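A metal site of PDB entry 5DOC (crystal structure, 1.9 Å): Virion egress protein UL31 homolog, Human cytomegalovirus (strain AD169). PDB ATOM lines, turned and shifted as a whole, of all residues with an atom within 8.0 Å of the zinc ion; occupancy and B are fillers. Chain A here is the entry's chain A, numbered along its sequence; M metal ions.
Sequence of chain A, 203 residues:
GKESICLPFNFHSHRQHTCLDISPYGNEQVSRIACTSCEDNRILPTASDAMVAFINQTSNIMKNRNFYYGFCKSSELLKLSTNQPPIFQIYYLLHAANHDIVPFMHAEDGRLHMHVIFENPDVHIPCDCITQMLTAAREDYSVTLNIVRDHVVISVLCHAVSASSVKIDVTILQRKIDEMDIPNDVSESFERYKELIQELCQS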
ATOM      1  N   HIS A  17     -25.312  17.724   1.960  1.00  0.00           N
ATOM      2  CA  HIS A  17     -25.969  18.883   2.572  1.00  0.00           C
ATOM      3  C   HIS A  17     -25.084  20.123   2.693  1.00  0.00           C
ATOM      4  O   HIS A  17     -25.258  20.899   3.618  1.00  0.00           O
ATOM      5  CB  HIS A  17     -26.560  18.537   3.947  1.00  0.00           C
ATOM      6  CG  HIS A  17     -27.285  17.226   3.994  1.00  0.00           C
ATOM      7  ND1 HIS A  17     -28.249  16.878   3.070  1.00  0.00           N
ATOM      8  CD2 HIS A  17     -27.174  16.172   4.845  1.00  0.00           C
ATOM      9  CE1 HIS A  17     -28.709  15.667   3.358  1.00  0.00           C
ATOM     10  NE2 HIS A  17     -28.057  15.214   4.416  1.00  0.00           N
ATOM     11  N   THR A  18     -24.131  20.309   1.766  1.00  0.00           N
ATOM     12  CA  THR A  18     -23.347  21.560   1.701  1.00  0.00           C
ATOM     13  C   THR A  18     -23.494  22.250   0.342  1.00  0.00           C
ATOM     14  O   THR A  18     -23.713  21.581  -0.702  1.00  0.00           O
ATOM     15  CB  THR A  18     -21.837  21.320   1.954  1.00  0.00           C
ATOM     16  OG1 THR A  18     -21.286  20.471   0.955  1.00  0.00           O
ATOM     17  CG2 THR A  18     -21.588  20.690   3.339  1.00  0.00           C
ATOM     18  N   CYS A  19     -23.307  23.570   0.348  1.00  0.00           N
ATOM     19  CA  CYS A  19     -23.200  24.395  -0.851  1.00  0.00           C
ATOM     20  C   CYS A  19     -21.735  24.767  -1.057  1.00  0.00           C
ATOM     21  O   CYS A  19     -20.941  24.676  -0.129  1.00  0.00           O
ATOM     22  CB  CYS A  19     -24.030  25.678  -0.692  1.00  0.00           C
ATOM     23  SG  CYS A  19     -25.764  25.373  -0.297  1.00  0.00           S
ATOM     24  N   LEU A  20     -21.399  25.161  -2.282  1.00  0.00           N
ATOM     25  CA  LEU A  20     -20.078  25.722  -2.557  1.00  0.00           C
ATOM     26  C   LEU A  20     -20.179  27.212  -2.702  1.00  0.00           C
ATOM     27  O   LEU A  20     -21.120  27.759  -3.294  1.00  0.00           O
ATOM     28  CB  LEU A  20     -19.444  25.141  -3.808  1.00  0.00           C
ATOM     29  CG  LEU A  20     -19.245  23.654  -3.755  1.00  0.00           C
ATOM     30  CD1 LEU A  20     -18.488  23.208  -5.011  1.00  0.00           C
ATOM     31  CD2 LEU A  20     -18.468  23.253  -2.514  1.00  0.00           C
ATOM     32  N   ASP A  21     -19.222  27.908  -2.094  1.00  0.00           N
ATOM     33  CA  ASP A  21     -19.200  29.355  -2.190  1.00  0.00           C
ATOM     34  C   ASP A  21     -17.808  29.809  -2.567  1.00  0.00           C
ATOM     35  O   ASP A  21     -16.841  29.624  -1.815  1.00  0.00           O
ATOM     36  CB  ASP A  21     -19.666  30.010  -0.912  1.00  0.00           C
ATOM     37  CG  ASP A  21     -20.072  31.445  -1.141  1.00  0.00           C
ATOM     38  OD1 ASP A  21     -21.142  31.663  -1.748  1.00  0.00           O
ATOM     39  OD2 ASP A  21     -19.261  32.349  -0.805  1.00  0.00           O
ATOM     40  N   VAL A  30     -20.205  25.247   2.580  1.00  0.00           N
ATOM     41  CA  VAL A  30     -21.006  25.647   3.721  1.00  0.00           C
ATOM     42  C   VAL A  30     -22.228  24.728   3.920  1.00  0.00           C
ATOM     43  O   VAL A  30     -22.771  24.207   2.971  1.00  0.00           O
ATOM     44  CB  VAL A  30     -21.454  27.134   3.578  1.00  0.00           C
ATOM     45  CG1 VAL A  30     -22.361  27.332   2.398  1.00  0.00           C
ATOM     46  CG2 VAL A  30     -22.116  27.608   4.866  1.00  0.00           C
ATOM     47  N   SER A  31     -22.628  24.527   5.180  1.00  0.00           N
ATOM     48  CA  SER A  31     -23.866  23.854   5.501  1.00  0.00           C
ATOM     49  C   SER A  31     -25.046  24.516   4.761  1.00  0.00           C
ATOM     50  O   SER A  31     -25.269  25.709   4.868  1.00  0.00           O
ATOM     51  CB  SER A  31     -24.127  23.896   7.008  1.00  0.00           C
ATOM     52  OG  SER A  31     -25.500  23.689   7.270  1.00  0.00           O
ATOM     53  N   ARG A  32     -25.827  23.716   4.048  1.00  0.00           N
ATOM     54  CA  ARG A  32     -27.064  24.183   3.383  1.00  0.00           C
ATOM     55  C   ARG A  32     -28.063  24.850   4.382  1.00  0.00           C
ATOM     56  O   ARG A  32     -28.680  25.866   4.065  1.00  0.00           O
ATOM     57  CB  ARG A  32     -27.686  22.972   2.652  1.00  0.00           C
ATOM     58  CG  ARG A  32     -29.050  23.198   2.030  1.00  0.00           C
ATOM     59  CD  ARG A  32     -29.026  24.362   1.083  1.00  0.00           C
ATOM     60  NE  ARG A  32     -30.383  24.693   0.636  1.00  0.00           N
ATOM     61  CZ  ARG A  32     -31.276  25.367   1.368  1.00  0.00           C
ATOM     62  NH1 ARG A  32     -30.983  25.754   2.601  1.00  0.00           N
ATOM     63  NH2 ARG A  32     -32.478  25.645   0.877  1.00  0.00           N
ATOM     64  N   ILE A  33     -28.156  24.297   5.605  1.00  0.00           N
ATOM     65  CA  ILE A  33     -28.920  24.859   6.704  1.00  0.00           C
ATOM     66  C   ILE A  33     -28.494  26.283   7.081  1.00  0.00           C
ATOM     67  O   ILE A  33     -29.311  27.124   7.476  1.00  0.00           O
ATOM     68  CB  ILE A  33     -28.743  23.973   7.969  1.00  0.00           C
ATOM     69  CG1 ILE A  33     -29.313  22.570   7.763  1.00  0.00           C
ATOM     70  CG2 ILE A  33     -29.344  24.612   9.219  1.00  0.00           C
ATOM     71  CD1 ILE A  33     -30.589  22.513   6.963  1.00  0.00           C
ATOM     72  N   ALA A  34     -27.201  26.545   6.980  1.00  0.00           N
ATOM     73  CA  ALA A  34     -26.638  27.812   7.448  1.00  0.00           C
ATOM     74  C   ALA A  34     -26.444  28.773   6.298  1.00  0.00           C
ATOM     75  O   ALA A  34     -26.065  29.919   6.503  1.00  0.00           O
ATOM     76  CB  ALA A  34     -25.320  27.574   8.177  1.00  0.00           C
ATOM     77  N   CYS A  35     -26.687  28.313   5.078  1.00  0.00           N
ATOM     78  CA  CYS A  35     -26.375  29.093   3.898  1.00  0.00           C
ATOM     79  C   CYS A  35     -27.334  30.248   3.730  1.00  0.00           C
ATOM     80  O   CYS A  35     -28.559  30.032   3.633  1.00  0.00           O
ATOM     81  CB  CYS A  35     -26.438  28.200   2.666  1.00  0.00           C
ATOM     82  SG  CYS A  35     -26.089  29.081   1.155  1.00  0.00           S
ATOM     83  N   THR A  36     -26.799  31.465   3.649  1.00  0.00           N
ATOM     84  CA  THR A  36     -27.655  32.657   3.449  1.00  0.00           C
ATOM     85  C   THR A  36     -28.038  32.902   1.976  1.00  0.00           C
ATOM     86  O   THR A  36     -29.081  33.498   1.724  1.00  0.00           O
ATOM     87  CB  THR A  36     -27.016  33.926   4.057  1.00  0.00           C
ATOM     88  OG1 THR A  36     -25.642  34.026   3.688  1.00  0.00           O
ATOM     89  CG2 THR A  36     -27.114  33.870   5.562  1.00  0.00           C
ATOM     90  N   SER A  37     -27.239  32.432   1.018  1.00  0.00           N
ATOM     91  CA  SER A  37     -27.618  32.527  -0.395  1.00  0.00           C
ATOM     92  C   SER A  37     -28.828  31.650  -0.730  1.00  0.00           C
ATOM     93  O   SER A  37     -29.688  32.041  -1.516  1.00  0.00           O
ATOM     94  CB  SER A  37     -26.450  32.143  -1.310  1.00  0.00           C
ATOM     95  OG  SER A  37     -25.318  32.918  -1.020  1.00  0.00           O
ATOM     96  N   CYS A  38     -28.896  30.463  -0.136  1.00  0.00           N
ATOM     97  CA  CYS A  38     -30.037  29.558  -0.304  1.00  0.00           C
ATOM     98  C   CYS A  38     -31.186  29.882   0.682  1.00  0.00           C
ATOM     99  O   CYS A  38     -32.273  29.299   0.572  1.00  0.00           O
ATOM    100  CB  CYS A  38     -29.570  28.108  -0.104  1.00  0.00           C
ATOM    101  SG  CYS A  38     -28.479  27.517  -1.424  1.00  0.00           S
ATOM    102  N   HIS A 124     -22.076  31.057  -6.179  1.00  0.00           N
ATOM    103  CA  HIS A 124     -22.663  30.138  -5.230  1.00  0.00           C
ATOM    104  C   HIS A 124     -23.282  28.936  -5.943  1.00  0.00           C
ATOM    105  O   HIS A 124     -24.127  29.104  -6.817  1.00  0.00           O
ATOM    106  CB  HIS A 124     -23.704  30.824  -4.366  1.00  0.00           C
ATOM    107  CG  HIS A 124     -24.168  29.975  -3.230  1.00  0.00           C
ATOM    108  ND1 HIS A 124     -23.525  29.944  -2.013  1.00  0.00           N
ATOM    109  CD2 HIS A 124     -25.174  29.084  -3.141  1.00  0.00           C
ATOM    110  CE1 HIS A 124     -24.138  29.090  -1.215  1.00  0.00           C
ATOM    111  NE2 HIS A 124     -25.151  28.553  -1.876  1.00  0.00           N
ATOM    112  N   ILE A 125     -22.869  27.730  -5.554  1.00  0.00           N
ATOM    113  CA  ILE A 125     -23.432  26.477  -6.085  1.00  0.00           C
ATOM    114  C   ILE A 125     -24.280  25.777  -5.012  1.00  0.00           C
ATOM    115  O   ILE A 125     -23.719  25.197  -4.054  1.00  0.00           O
ATOM    116  CB  ILE A 125     -22.356  25.474  -6.598  1.00  0.00           C
ATOM    117  CG1 ILE A 125     -21.249  26.142  -7.432  1.00  0.00           C
ATOM    118  CG2 ILE A 125     -23.024  24.344  -7.369  1.00  0.00           C
ATOM    119  CD1 ILE A 125     -21.707  26.754  -8.749  1.00  0.00           C
ATOM    120  N   PRO A 126     -25.628  25.846  -5.152  1.00  0.00           N
ATOM    121  CA  PRO A 126     -26.509  25.329  -4.114  1.00  0.00           C
ATOM    122  C   PRO A 126     -26.375  23.835  -3.986  1.00  0.00           C
ATOM    123  O   PRO A 126     -26.124  23.148  -4.971  1.00  0.00           O
ATOM    124  CB  PRO A 126     -27.913  25.675  -4.625  1.00  0.00           C
ATOM    125  CG  PRO A 126     -27.758  26.720  -5.637  1.00  0.00           C
ATOM    126  CD  PRO A 126     -26.391  26.527  -6.226  1.00  0.00           C
ATOM    127  N   CYS A 127     -26.497  23.351  -2.744  1.00  0.00           N
ATOM    128  CA  CYS A 127     -26.435  21.923  -2.495  1.00  0.00           C
ATOM    129  C   CYS A 127     -27.342  21.145  -3.461  1.00  0.00           C
ATOM    130  O   CYS A 127     -26.956  20.101  -4.020  1.00  0.00           O
ATOM    131  CB  CYS A 127     -26.889  21.640  -1.057  1.00  0.00           C
ATOM    132  SG  CYS A 127     -26.696  19.906  -0.644  1.00  0.00           S
ATOM    133  N   ASP A 128     -28.543  21.649  -3.653  1.00  0.00           N
ATOM    134  CA  ASP A 128     -29.547  20.937  -4.436  1.00  0.00           C
ATOM    135  C   ASP A 128     -29.129  20.791  -5.917  1.00  0.00           C
ATOM    136  O   ASP A 128     -29.417  19.769  -6.557  1.00  0.00           O
ATOM    137  CB  ASP A 128     -30.888  21.645  -4.331  1.00  0.00           C
ATOM    138  CG  ASP A 128     -31.550  21.415  -2.985  1.00  0.00           C
ATOM    139  OD1 ASP A 128     -31.316  20.334  -2.399  1.00  0.00           O
ATOM    140  OD2 ASP A 128     -32.305  22.311  -2.506  1.00  0.00           O
HETATM  141 ZN    ZN M   1     -26.411  27.537  -0.519  1.00  0.00          ZN
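A ring nitrogen (ND1) of His 124 lies within hydrogen-bond range of the side-chain carboxylate of Asp 21, 3.0 Å away.
The side-chain sulfur of Cys 19 lies close to the backbone NH of Cys 127 (3.3 Å).
The side-chain sulfur of Cys 35 lies close to the backbone NH of Ser 37 (3.5 Å).
N of Cys 19 is in hydrogen-bond range of O of Val 30, at 2.8 Å.
ND1 of His 124 sits close to O of Leu 20 (3.5 Å).
Of the 19 residues printed, 4 come within 4 Å of the zinc ion.
The zinc ion is bound by NE2 of His 124 (2.1 Å), SG of Cys 38 (2.3 Å), SG of Cys 19 (2.3 Å) and SG of Cys 35 (2.3 Å).
The zinc ion has four donor atoms within binding distance.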
